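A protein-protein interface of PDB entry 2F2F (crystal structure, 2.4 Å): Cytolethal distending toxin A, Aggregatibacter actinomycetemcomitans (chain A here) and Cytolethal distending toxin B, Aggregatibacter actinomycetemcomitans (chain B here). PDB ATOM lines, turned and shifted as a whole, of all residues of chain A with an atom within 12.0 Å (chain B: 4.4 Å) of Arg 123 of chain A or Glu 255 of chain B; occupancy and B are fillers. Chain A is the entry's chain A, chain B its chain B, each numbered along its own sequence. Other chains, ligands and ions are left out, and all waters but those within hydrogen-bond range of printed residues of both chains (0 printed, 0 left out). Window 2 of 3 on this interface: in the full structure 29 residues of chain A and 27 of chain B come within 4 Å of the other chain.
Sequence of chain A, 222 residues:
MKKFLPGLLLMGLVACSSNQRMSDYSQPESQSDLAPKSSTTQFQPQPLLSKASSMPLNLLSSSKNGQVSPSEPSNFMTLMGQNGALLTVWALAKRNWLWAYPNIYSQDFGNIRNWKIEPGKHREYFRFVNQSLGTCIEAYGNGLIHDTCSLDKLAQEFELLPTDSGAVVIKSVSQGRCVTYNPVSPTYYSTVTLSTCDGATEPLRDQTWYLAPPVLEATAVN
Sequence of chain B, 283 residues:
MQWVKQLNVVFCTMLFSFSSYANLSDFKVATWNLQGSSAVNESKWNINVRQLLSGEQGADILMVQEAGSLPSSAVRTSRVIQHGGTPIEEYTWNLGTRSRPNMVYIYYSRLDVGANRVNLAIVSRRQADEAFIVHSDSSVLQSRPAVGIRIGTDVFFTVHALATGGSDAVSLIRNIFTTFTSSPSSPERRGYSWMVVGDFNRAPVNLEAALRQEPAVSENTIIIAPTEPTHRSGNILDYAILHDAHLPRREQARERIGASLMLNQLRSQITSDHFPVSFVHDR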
ATOM      1  N   ILE A 117       3.761  26.610 -19.745  1.00  0.00           N
ATOM      2  CA  ILE A 117       3.534  26.160 -18.367  1.00  0.00           C
ATOM      3  C   ILE A 117       3.003  24.725 -18.389  1.00  0.00           C
ATOM      4  O   ILE A 117       1.980  24.438 -19.005  1.00  0.00           O
ATOM      5  CB  ILE A 117       2.495  27.008 -17.636  1.00  0.00           C
ATOM      6  CG1 ILE A 117       2.856  28.486 -17.743  1.00  0.00           C
ATOM      7  CG2 ILE A 117       2.452  26.590 -16.180  1.00  0.00           C
ATOM      8  CD1 ILE A 117       1.882  29.392 -16.996  1.00  0.00           C
ATOM      9  N   GLU A 118       3.728  23.825 -17.738  1.00  0.00           N
ATOM     10  CA  GLU A 118       3.355  22.424 -17.677  1.00  0.00           C
ATOM     11  C   GLU A 118       3.212  22.005 -16.237  1.00  0.00           C
ATOM     12  O   GLU A 118       3.629  22.721 -15.324  1.00  0.00           O
ATOM     13  CB  GLU A 118       4.440  21.558 -18.306  1.00  0.00           C
ATOM     14  CG  GLU A 118       4.555  21.707 -19.795  1.00  0.00           C
ATOM     15  CD  GLU A 118       5.627  20.815 -20.365  1.00  0.00           C
ATOM     16  OE1 GLU A 118       6.421  20.277 -19.565  1.00  0.00           O
ATOM     17  OE2 GLU A 118       5.670  20.648 -21.602  1.00  0.00           O
ATOM     18  N   PRO A 119       2.590  20.848 -15.998  1.00  0.00           N
ATOM     19  CA  PRO A 119       2.450  20.427 -14.603  1.00  0.00           C
ATOM     20  C   PRO A 119       3.805  19.916 -14.089  1.00  0.00           C
ATOM     21  O   PRO A 119       4.547  19.254 -14.811  1.00  0.00           O
ATOM     22  CB  PRO A 119       1.389  19.322 -14.651  1.00  0.00           C
ATOM     23  CG  PRO A 119       0.935  19.239 -16.098  1.00  0.00           C
ATOM     24  CD  PRO A 119       1.978  19.892 -16.934  1.00  0.00           C
ATOM     25  N   GLY A 120       4.130  20.232 -12.845  1.00  0.00           N
ATOM     26  CA  GLY A 120       5.395  19.765 -12.316  1.00  0.00           C
ATOM     27  C   GLY A 120       5.360  18.265 -12.079  1.00  0.00           C
ATOM     28  O   GLY A 120       4.518  17.552 -12.615  1.00  0.00           O
ATOM     29  N   LYS A 121       6.322  17.785 -11.310  1.00  0.00           N
ATOM     30  CA  LYS A 121       6.393  16.386 -10.963  1.00  0.00           C
ATOM     31  C   LYS A 121       5.266  16.146  -9.967  1.00  0.00           C
ATOM     32  O   LYS A 121       4.629  15.094  -9.979  1.00  0.00           O
ATOM     33  CB  LYS A 121       7.744  16.068 -10.315  1.00  0.00           C
ATOM     34  CG  LYS A 121       7.894  14.650  -9.778  1.00  0.00           C
ATOM     35  CD  LYS A 121       9.214  14.507  -9.038  1.00  0.00           C
ATOM     36  CE  LYS A 121       9.477  13.080  -8.597  1.00  0.00           C
ATOM     37  NZ  LYS A 121      10.646  13.013  -7.673  1.00  0.00           N
ATOM     38  N   HIS A 122       5.033  17.145  -9.115  1.00  0.00           N
ATOM     39  CA  HIS A 122       4.007  17.103  -8.078  1.00  0.00           C
ATOM     40  C   HIS A 122       2.718  17.777  -8.547  1.00  0.00           C
ATOM     41  O   HIS A 122       2.752  18.742  -9.315  1.00  0.00           O
ATOM     42  CB  HIS A 122       4.537  17.776  -6.815  1.00  0.00           C
ATOM     43  CG  HIS A 122       5.759  17.117  -6.261  1.00  0.00           C
ATOM     44  ND1 HIS A 122       7.038  17.553  -6.544  1.00  0.00           N
ATOM     45  CD2 HIS A 122       5.902  16.046  -5.446  1.00  0.00           C
ATOM     46  CE1 HIS A 122       7.911  16.778  -5.929  1.00  0.00           C
ATOM     47  NE2 HIS A 122       7.250  15.854  -5.257  1.00  0.00           N
ATOM     48  N   ARG A 123       1.591  17.252  -8.065  1.00  0.00           N
ATOM     49  CA  ARG A 123       0.240  17.688  -8.439  1.00  0.00           C
ATOM     50  C   ARG A 123      -0.144  19.147  -8.715  1.00  0.00           C
ATOM     51  O   ARG A 123      -0.535  19.483  -9.843  1.00  0.00           O
ATOM     52  CB  ARG A 123      -0.781  17.072  -7.472  1.00  0.00           C
ATOM     53  CG  ARG A 123      -1.449  15.826  -8.073  1.00  0.00           C
ATOM     54  CD  ARG A 123      -2.270  15.024  -7.073  1.00  0.00           C
ATOM     55  NE  ARG A 123      -2.461  13.641  -7.509  1.00  0.00           N
ATOM     56  CZ  ARG A 123      -3.277  12.769  -6.915  1.00  0.00           C
ATOM     57  NH1 ARG A 123      -3.989  13.128  -5.853  1.00  0.00           N
ATOM     58  NH2 ARG A 123      -3.380  11.533  -7.383  1.00  0.00           N
ATOM     59  N   GLU A 124      -0.084  20.016  -7.715  1.00  0.00           N
ATOM     60  CA  GLU A 124      -0.469  21.398  -7.967  1.00  0.00           C
ATOM     61  C   GLU A 124       0.672  22.342  -8.367  1.00  0.00           C
ATOM     62  O   GLU A 124       0.482  23.557  -8.400  1.00  0.00           O
ATOM     63  CB  GLU A 124      -1.224  21.946  -6.759  1.00  0.00           C
ATOM     64  CG  GLU A 124      -2.587  21.302  -6.572  1.00  0.00           C
ATOM     65  CD  GLU A 124      -3.260  21.710  -5.285  1.00  0.00           C
ATOM     66  OE1 GLU A 124      -2.903  21.159  -4.222  1.00  0.00           O
ATOM     67  OE2 GLU A 124      -4.150  22.586  -5.338  1.00  0.00           O
ATOM     68  N   TYR A 125       1.845  21.778  -8.674  1.00  0.00           N
ATOM     69  CA  TYR A 125       3.011  22.560  -9.072  1.00  0.00           C
ATOM     70  C   TYR A 125       3.183  22.632 -10.576  1.00  0.00           C
ATOM     71  O   TYR A 125       2.672  21.803 -11.311  1.00  0.00           O
ATOM     72  CB  TYR A 125       4.266  21.968  -8.450  1.00  0.00           C
ATOM     73  CG  TYR A 125       4.221  21.970  -6.949  1.00  0.00           C
ATOM     74  CD1 TYR A 125       3.296  22.750  -6.266  1.00  0.00           C
ATOM     75  CD2 TYR A 125       5.098  21.193  -6.208  1.00  0.00           C
ATOM     76  CE1 TYR A 125       3.245  22.757  -4.881  1.00  0.00           C
ATOM     77  CE2 TYR A 125       5.055  21.194  -4.819  1.00  0.00           C
ATOM     78  CZ  TYR A 125       4.126  21.979  -4.164  1.00  0.00           C
ATOM     79  OH  TYR A 125       4.096  22.000  -2.794  1.00  0.00           O
ATOM     80  N   PHE A 126       3.920  23.636 -11.021  1.00  0.00           N
ATOM     81  CA  PHE A 126       4.165  23.845 -12.433  1.00  0.00           C
ATOM     82  C   PHE A 126       5.632  24.146 -12.659  1.00  0.00           C
ATOM     83  O   PHE A 126       6.377  24.438 -11.729  1.00  0.00           O
ATOM     84  CB  PHE A 126       3.352  25.036 -12.946  1.00  0.00           C
ATOM     85  CG  PHE A 126       1.873  24.817 -12.929  1.00  0.00           C
ATOM     86  CD1 PHE A 126       1.252  24.110 -13.955  1.00  0.00           C
ATOM     87  CD2 PHE A 126       1.099  25.323 -11.891  1.00  0.00           C
ATOM     88  CE1 PHE A 126      -0.127  23.906 -13.950  1.00  0.00           C
ATOM     89  CE2 PHE A 126      -0.280  25.129 -11.871  1.00  0.00           C
ATOM     90  CZ  PHE A 126      -0.896  24.418 -12.904  1.00  0.00           C
ATOM     91  N   ARG A 127       6.034  24.063 -13.914  1.00  0.00           N
ATOM     92  CA  ARG A 127       7.391  24.358 -14.331  1.00  0.00           C
ATOM     93  C   ARG A 127       7.218  25.190 -15.594  1.00  0.00           C
ATOM     94  O   ARG A 127       6.178  25.118 -16.236  1.00  0.00           O
ATOM     95  CB  ARG A 127       8.143  23.057 -14.637  1.00  0.00           C
ATOM     96  CG  ARG A 127       7.627  22.296 -15.860  1.00  0.00           C
ATOM     97  CD  ARG A 127       8.355  20.972 -15.996  1.00  0.00           C
ATOM     98  NE  ARG A 127       8.132  20.329 -17.292  1.00  0.00           N
ATOM     99  CZ  ARG A 127       8.841  19.288 -17.724  1.00  0.00           C
ATOM    100  NH1 ARG A 127       9.811  18.788 -16.963  1.00  0.00           N
ATOM    101  NH2 ARG A 127       8.577  18.733 -18.896  1.00  0.00           N
ATOM    102  N   LEU A 151      12.408  16.683 -14.154  1.00  0.00           N
ATOM    103  CA  LEU A 151      11.265  16.560 -13.250  1.00  0.00           C
ATOM    104  C   LEU A 151      11.627  16.293 -11.801  1.00  0.00           C
ATOM    105  O   LEU A 151      10.824  16.544 -10.895  1.00  0.00           O
ATOM    106  CB  LEU A 151      10.305  15.486 -13.753  1.00  0.00           C
ATOM    107  CG  LEU A 151       9.504  15.933 -14.975  1.00  0.00           C
ATOM    108  CD1 LEU A 151       8.904  14.712 -15.638  1.00  0.00           C
ATOM    109  CD2 LEU A 151       8.428  16.946 -14.576  1.00  0.00           C
ATOM    110  N   ASP A 152      12.837  15.805 -11.577  1.00  0.00           N
ATOM    111  CA  ASP A 152      13.270  15.505 -10.226  1.00  0.00           C
ATOM    112  C   ASP A 152      13.919  16.680  -9.513  1.00  0.00           C
ATOM    113  O   ASP A 152      14.224  16.602  -8.322  1.00  0.00           O
ATOM    114  CB  ASP A 152      14.191  14.290 -10.251  1.00  0.00           C
ATOM    115  CG  ASP A 152      13.446  13.028 -10.653  1.00  0.00           C
ATOM    116  OD1 ASP A 152      12.634  12.530  -9.829  1.00  0.00           O
ATOM    117  OD2 ASP A 152      13.656  12.554 -11.794  1.00  0.00           O
ATOM    118  N   LYS A 153      14.127  17.773 -10.242  1.00  0.00           N
ATOM    119  CA  LYS A 153      14.697  18.970  -9.638  1.00  0.00           C
ATOM    120  C   LYS A 153      13.532  19.779  -9.064  1.00  0.00           C
ATOM    121  O   LYS A 153      12.752  20.382  -9.806  1.00  0.00           O
ATOM    122  CB  LYS A 153      15.455  19.802 -10.680  1.00  0.00           C
ATOM    123  CG  LYS A 153      16.705  19.138 -11.271  1.00  0.00           C
ATOM    124  CD  LYS A 153      17.391  20.073 -12.265  1.00  0.00           C
ATOM    125  CE  LYS A 153      18.397  19.365 -13.173  1.00  0.00           C
ATOM    126  NZ  LYS A 153      18.784  20.226 -14.344  1.00  0.00           N
ATOM    127  N   LEU A 154      13.388  19.755  -7.746  1.00  0.00           N
ATOM    128  CA  LEU A 154      12.319  20.495  -7.093  1.00  0.00           C
ATOM    129  C   LEU A 154      12.431  22.003  -7.339  1.00  0.00           C
ATOM    130  O   LEU A 154      11.428  22.693  -7.498  1.00  0.00           O
ATOM    131  CB  LEU A 154      12.327  20.210  -5.583  1.00  0.00           C
ATOM    132  CG  LEU A 154      11.082  20.690  -4.819  1.00  0.00           C
ATOM    133  CD1 LEU A 154       9.903  19.780  -5.121  1.00  0.00           C
ATOM    134  CD2 LEU A 154      11.367  20.727  -3.331  1.00  0.00           C
ATOM    135  N   GLN A 156      12.796  23.489  -9.756  1.00  0.00           N
ATOM    136  CA  GLN A 156      12.173  23.837 -11.032  1.00  0.00           C
ATOM    137  C   GLN A 156      10.642  23.802 -10.999  1.00  0.00           C
ATOM    138  O   GLN A 156       9.976  23.936 -12.030  1.00  0.00           O
ATOM    139  CB  GLN A 156      12.688  22.911 -12.138  1.00  0.00           C
ATOM    140  CG  GLN A 156      14.116  23.223 -12.552  1.00  0.00           C
ATOM    141  CD  GLN A 156      14.586  22.436 -13.762  1.00  0.00           C
ATOM    142  OE1 GLN A 156      13.815  21.702 -14.380  1.00  0.00           O
ATOM    143  NE2 GLN A 156      15.872  22.584 -14.104  1.00  0.00           N
ATOM    144  N   GLU A 157      10.091  23.627  -9.803  1.00  0.00           N
ATOM    145  CA  GLU A 157       8.643  23.579  -9.619  1.00  0.00           C
ATOM    146  C   GLU A 157       8.145  24.804  -8.859  1.00  0.00           C
ATOM    147  O   GLU A 157       8.669  25.147  -7.796  1.00  0.00           O
ATOM    148  CB  GLU A 157       8.259  22.314  -8.857  1.00  0.00           C
ATOM    149  CG  GLU A 157       8.306  21.052  -9.693  1.00  0.00           C
ATOM    150  CD  GLU A 157       7.637  19.903  -8.984  1.00  0.00           C
ATOM    151  OE1 GLU A 157       6.546  19.495  -9.429  1.00  0.00           O
ATOM    152  OE2 GLU A 157       8.191  19.421  -7.974  1.00  0.00           O
ATOM    153  N   PHE A 158       7.102  25.432  -9.392  1.00  0.00           N
ATOM    154  CA  PHE A 158       6.546  26.630  -8.774  1.00  0.00           C
ATOM    155  C   PHE A 158       5.039  26.560  -8.547  1.00  0.00           C
ATOM    156  O   PHE A 158       4.315  25.823  -9.217  1.00  0.00           O
ATOM    157  CB  PHE A 158       6.837  27.862  -9.652  1.00  0.00           C
ATOM    158  CG  PHE A 158       8.300  28.169  -9.812  1.00  0.00           C
ATOM    159  CD1 PHE A 158       8.956  28.975  -8.898  1.00  0.00           C
ATOM    160  CD2 PHE A 158       9.024  27.632 -10.872  1.00  0.00           C
ATOM    161  CE1 PHE A 158      10.322  29.246  -9.030  1.00  0.00           C
ATOM    162  CE2 PHE A 158      10.388  27.897 -11.010  1.00  0.00           C
ATOM    163  CZ  PHE A 158      11.035  28.706 -10.088  1.00  0.00           C
ATOM    164  N   GLU A 159       4.575  27.387  -7.621  1.00  0.00           N
ATOM    165  CA  GLU A 159       3.168  27.477  -7.300  1.00  0.00           C
ATOM    166  C   GLU A 159       2.683  28.785  -7.910  1.00  0.00           C
ATOM    167  O   GLU A 159       3.355  29.808  -7.813  1.00  0.00           O
ATOM    168  CB  GLU A 159       2.981  27.563  -5.792  1.00  0.00           C
ATOM    169  CG  GLU A 159       3.008  26.254  -5.057  1.00  0.00           C
ATOM    170  CD  GLU A 159       2.737  26.443  -3.583  1.00  0.00           C
ATOM    171  OE1 GLU A 159       1.542  26.538  -3.208  1.00  0.00           O
ATOM    172  OE2 GLU A 159       3.719  26.510  -2.805  1.00  0.00           O
ATOM    173  N   LEU A 160       1.504  28.761  -8.512  1.00  0.00           N
ATOM    174  CA  LEU A 160       0.936  29.958  -9.098  1.00  0.00           C
ATOM    175  C   LEU A 160      -0.223  30.300  -8.159  1.00  0.00           C
ATOM    176  O   LEU A 160      -1.318  29.767  -8.295  1.00  0.00           O
ATOM    177  CB  LEU A 160       0.426  29.655 -10.508  1.00  0.00           C
ATOM    178  CG  LEU A 160       1.454  29.540 -11.634  1.00  0.00           C
ATOM    179  CD1 LEU A 160       0.734  29.310 -12.942  1.00  0.00           C
ATOM    180  CD2 LEU A 160       2.298  30.811 -11.712  1.00  0.00           C
ATOM    181  N   LEU A 161       0.043  31.205  -7.219  1.00  0.00           N
ATOM    182  CA  LEU A 161      -0.918  31.621  -6.197  1.00  0.00           C
ATOM    183  C   LEU A 161      -1.865  32.694  -6.700  1.00  0.00           C
ATOM    184  O   LEU A 161      -1.440  33.732  -7.198  1.00  0.00           O
ATOM    185  CB  LEU A 161      -0.186  32.137  -4.956  1.00  0.00           C
ATOM    186  CG  LEU A 161       0.951  31.290  -4.382  1.00  0.00           C
ATOM    187  CD1 LEU A 161       1.541  31.969  -3.154  1.00  0.00           C
ATOM    188  CD2 LEU A 161       0.432  29.940  -4.002  1.00  0.00           C
ATOM    189  N   VAL A 173       8.713  26.373  -4.958  1.00  0.00           N
ATOM    190  CA  VAL A 173       8.433  25.246  -4.078  1.00  0.00           C
ATOM    191  C   VAL A 173       9.673  24.897  -3.254  1.00  0.00           C
ATOM    192  O   VAL A 173       9.593  24.691  -2.047  1.00  0.00           O
ATOM    193  CB  VAL A 173       7.988  24.000  -4.896  1.00  0.00           C
ATOM    194  CG1 VAL A 173       7.977  22.758  -4.018  1.00  0.00           C
ATOM    195  CG2 VAL A 173       6.616  24.240  -5.487  1.00  0.00           C
ATOM    196  N   SER B  25      -9.440   8.842 -16.057  1.00  0.00           N
ATOM    197  CA  SER B  25      -8.069   9.332 -16.135  1.00  0.00           C
ATOM    198  C   SER B  25      -7.564   9.537 -17.552  1.00  0.00           C
ATOM    199  O   SER B  25      -6.470  10.044 -17.739  1.00  0.00           O
ATOM    200  CB  SER B  25      -7.136   8.391 -15.369  1.00  0.00           C
ATOM    201  OG  SER B  25      -6.994   7.150 -16.038  1.00  0.00           O
ATOM    202  N   LEU B 242     -15.486  11.328  -7.453  1.00  0.00           N
ATOM    203  CA  LEU B 242     -15.651  10.311  -8.478  1.00  0.00           C
ATOM    204  C   LEU B 242     -15.709   8.884  -7.991  1.00  0.00           C
ATOM    205  O   LEU B 242     -15.364   8.562  -6.843  1.00  0.00           O
ATOM    206  CB  LEU B 242     -14.526  10.439  -9.529  1.00  0.00           C
ATOM    207  CG  LEU B 242     -13.067  10.168  -9.122  1.00  0.00           C
ATOM    208  CD1 LEU B 242     -12.834   8.680  -8.936  1.00  0.00           C
ATOM    209  CD2 LEU B 242     -12.131  10.722 -10.188  1.00  0.00           C
ATOM    210  N   ASP B 244     -14.446   5.198  -9.592  1.00  0.00           N
ATOM    211  CA  ASP B 244     -13.757   4.432 -10.631  1.00  0.00           C
ATOM    212  C   ASP B 244     -14.268   2.993 -10.530  1.00  0.00           C
ATOM    213  O   ASP B 244     -14.005   2.304  -9.538  1.00  0.00           O
ATOM    214  CB  ASP B 244     -12.246   4.429 -10.386  1.00  0.00           C
ATOM    215  CG  ASP B 244     -11.454   3.886 -11.569  1.00  0.00           C
ATOM    216  OD1 ASP B 244     -11.996   3.113 -12.389  1.00  0.00           O
ATOM    217  OD2 ASP B 244     -10.274   4.246 -11.689  1.00  0.00           O
ATOM    218  N   LEU B 247     -11.814   0.247  -9.659  1.00  0.00           N
ATOM    219  CA  LEU B 247     -11.123   0.300  -8.383  1.00  0.00           C
ATOM    220  C   LEU B 247     -12.095  -0.290  -7.368  1.00  0.00           C
ATOM    221  O   LEU B 247     -13.289  -0.006  -7.380  1.00  0.00           O
ATOM    222  CB  LEU B 247     -10.750   1.735  -8.013  1.00  0.00           C
ATOM    223  CG  LEU B 247      -9.508   2.298  -8.703  1.00  0.00           C
ATOM    224  CD1 LEU B 247      -9.226   3.679  -8.159  1.00  0.00           C
ATOM    225  CD2 LEU B 247      -8.319   1.405  -8.446  1.00  0.00           C
ATOM    226  N   GLN B 252     -10.755   3.684  -3.827  1.00  0.00           N
ATOM    227  CA  GLN B 252     -10.842   4.743  -4.811  1.00  0.00           C
ATOM    228  C   GLN B 252      -9.669   5.715  -4.686  1.00  0.00           C
ATOM    229  O   GLN B 252      -9.286   6.353  -5.663  1.00  0.00           O
ATOM    230  CB  GLN B 252     -12.160   5.505  -4.654  1.00  0.00           C
ATOM    231  CG  GLN B 252     -13.380   4.657  -4.886  1.00  0.00           C
ATOM    232  CD  GLN B 252     -13.515   4.235  -6.316  1.00  0.00           C
ATOM    233  OE1 GLN B 252     -13.469   5.059  -7.226  1.00  0.00           O
ATOM    234  NE2 GLN B 252     -13.689   2.934  -6.532  1.00  0.00           N
ATOM    235  N   ALA B 253      -9.099   5.823  -3.491  1.00  0.00           N
ATOM    236  CA  ALA B 253      -7.981   6.736  -3.261  1.00  0.00           C
ATOM    237  C   ALA B 253      -6.749   6.346  -4.045  1.00  0.00           C
ATOM    238  O   ALA B 253      -5.743   7.051  -4.010  1.00  0.00           O
ATOM    239  CB  ALA B 253      -7.637   6.789  -1.788  1.00  0.00           C
ATOM    240  N   ARG B 254      -6.820   5.209  -4.729  1.00  0.00           N
ATOM    241  CA  ARG B 254      -5.704   4.730  -5.539  1.00  0.00           C
ATOM    242  C   ARG B 254      -5.724   5.498  -6.844  1.00  0.00           C
ATOM    243  O   ARG B 254      -4.777   5.428  -7.615  1.00  0.00           O
ATOM    244  CB  ARG B 254      -5.862   3.236  -5.844  1.00  0.00           C
ATOM    245  CG  ARG B 254      -5.515   2.293  -4.709  1.00  0.00           C
ATOM    246  CD  ARG B 254      -5.156   0.900  -5.244  1.00  0.00           C
ATOM    247  NE  ARG B 254      -4.395   0.137  -4.256  1.00  0.00           N
ATOM    248  CZ  ARG B 254      -3.147   0.418  -3.880  1.00  0.00           C
ATOM    249  NH1 ARG B 254      -2.552  -0.340  -2.965  1.00  0.00           N
ATOM    250  NH2 ARG B 254      -2.485   1.445  -4.416  1.00  0.00           N
ATOM    251  N   GLU B 255      -6.818   6.211  -7.100  1.00  0.00           N
ATOM    252  CA  GLU B 255      -6.938   6.964  -8.342  1.00  0.00           C
ATOM    253  C   GLU B 255      -5.747   7.901  -8.598  1.00  0.00           C
ATOM    254  O   GLU B 255      -5.292   8.646  -7.722  1.00  0.00           O
ATOM    255  CB  GLU B 255      -8.258   7.755  -8.366  1.00  0.00           C
ATOM    256  CG  GLU B 255      -8.606   8.342  -9.733  1.00  0.00           C
ATOM    257  CD  GLU B 255      -9.063   7.292 -10.732  1.00  0.00           C
ATOM    258  OE1 GLU B 255      -9.724   6.324 -10.310  1.00  0.00           O
ATOM    259  OE2 GLU B 255      -8.772   7.423 -11.938  1.00  0.00           O
ATOM    260  N   ARG B 256      -5.281   7.859  -9.839  1.00  0.00           N
ATOM    261  CA  ARG B 256      -4.148   8.641 -10.298  1.00  0.00           C
ATOM    262  C   ARG B 256      -4.631   9.903 -10.991  1.00  0.00           C
ATOM    263  O   ARG B 256      -4.181  10.234 -12.081  1.00  0.00           O
ATOM    264  CB  ARG B 256      -3.310   7.806 -11.267  1.00  0.00           C
ATOM    265  CG  ARG B 256      -2.839   6.496 -10.672  1.00  0.00           C
ATOM    266  CD  ARG B 256      -1.902   6.731  -9.502  1.00  0.00           C
ATOM    267  NE  ARG B 256      -0.561   7.106  -9.948  1.00  0.00           N
ATOM    268  CZ  ARG B 256       0.210   6.363 -10.745  1.00  0.00           C
ATOM    269  NH1 ARG B 256      -0.215   5.182 -11.197  1.00  0.00           N
ATOM    270  NH2 ARG B 256       1.410   6.812 -11.099  1.00  0.00           N
ATOM    271  N   ILE B 257      -5.629  10.545 -10.400  1.00  0.00           N
ATOM    272  CA  ILE B 257      -6.145  11.787 -10.935  1.00  0.00           C
ATOM    273  C   ILE B 257      -5.956  12.839  -9.863  1.00  0.00           C
ATOM    274  O   ILE B 257      -6.256  12.607  -8.690  1.00  0.00           O
ATOM    275  CB  ILE B 257      -7.625  11.686 -11.301  1.00  0.00           C
ATOM    276  CG1 ILE B 257      -7.797  10.608 -12.359  1.00  0.00           C
ATOM    277  CG2 ILE B 257      -8.142  13.033 -11.764  1.00  0.00           C
ATOM    278  CD1 ILE B 257      -8.778  10.910 -13.388  1.00  0.00           C
ATOM    279  N   GLY B 258      -5.381  13.967 -10.259  1.00  0.00           N
ATOM    280  CA  GLY B 258      -5.135  15.044  -9.314  1.00  0.00           C
ATOM    281  C   GLY B 258      -5.843  16.306  -9.745  1.00  0.00           C
ATOM    282  O   GLY B 258      -6.054  16.518 -10.933  1.00  0.00           O
ATOM    283  N   SER B 260      -6.181  20.642  -9.571  1.00  0.00           N
ATOM    284  CA  SER B 260      -5.408  21.852  -9.349  1.00  0.00           C
ATOM    285  C   SER B 260      -5.999  23.010 -10.132  1.00  0.00           C
ATOM    286  O   SER B 260      -6.730  22.795 -11.086  1.00  0.00           O
ATOM    287  CB  SER B 260      -3.952  21.635  -9.769  1.00  0.00           C
ATOM    288  OG  SER B 260      -3.775  21.882 -11.150  1.00  0.00           O
ATOM    289  N   ASP B 282      -2.067  11.787 -13.168  1.00  0.00           N
ATOM    290  CA  ASP B 282      -0.743  12.046 -12.607  1.00  0.00           C
ATOM    291  C   ASP B 282       0.303  11.583 -13.616  1.00  0.00           C
ATOM    292  O   ASP B 282       0.391  10.392 -13.917  1.00  0.00           O
ATOM    293  CB  ASP B 282      -0.544  11.246 -11.316  1.00  0.00           C
ATOM    294  CG  ASP B 282      -1.312  11.811 -10.155  1.00  0.00           C
ATOM    295  OD1 ASP B 282      -1.636  13.013 -10.188  1.00  0.00           O
ATOM    296  OD2 ASP B 282      -1.595  11.056  -9.201  1.00  0.00           O
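Of chain B, only Glu 255 (3.5 Å), Ile 257 (3.3 Å), Gly 258 (3.5 Å) and Asp 282 (2.6 Å) come within 4 Å of Arg 123 of chain A.
Of the printed residues of chain B, Glu 124 of chain A touches Ser 260.
Glu 157 of chain A touches none of the printed residues of chain B.
No residue of chain A comes within 4 Å of Ser 25 of chain B.
No residue of chain A comes within 4 Å of Leu 247 of chain B.
Of the printed residues of chain A, Glu 255 of chain B touches Arg 123.
No residue of chain A comes within 4 Å of Arg 256 of chain B.
Ile 257 of chain B touches just one residue of chain A: Arg 123.
Of chain A, only Arg 123 comes within 4 Å of Gly 258 of chain B.
Of chain A, only Glu 124 comes within 4 Å of Ser 260 of chain B.
Of chain A, only Arg 123 comes within 4 Å of Asp 282 of chain B.
The nearest residue of chain B that does not touch Arg 123 of chain A is Ser 260 of chain B (4.04 Å).
Arg 123 of chain A touches Gly 258 of chain B (NE to CA, 3.5 Å).
Glu 124 of chain A touches Ser 260 of chain B.
NH2 of Arg 123 of chain A sits at hydrogen-bond distance from O of Glu 255 of chain B (3.5 Å).
The guanidinium group (NH2) of Arg 123 of chain A sits at hydrogen-bond distance from the backbone carbonyl oxygen (O) of Ile 257 of chain B, 3.3 Å away.
OD2 of Asp 282 of chain B is in salt-bridge range of NH2 of Arg 123 of chain A, 2.6 Å away.
OE1 of Glu 255 of chain B sits close to OD2 of Asp 244 of chain B, 2.6 Å away.
O of Arg 256 of chain B lies within hydrogen-bond range of N of Asp 282 of chain B.
Of the 13 printed residues of chain B, 5 touch a printed residue of chain A.
Of the 22 printed residues of chain A, 2 touch a printed residue of chain B.
Printed residues of chain A that touch a printed residue of chain B: Arg 123 and Glu 124.
Among the printed residues, 5 pairs touch across the chains.
Among the printed residues, Asp or Glu carboxylates within 4 Å of a Lys or Arg side-chain nitrogen of the other chain: Arg 123 of chain A with Asp 282 of chain B (2.6 Å).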
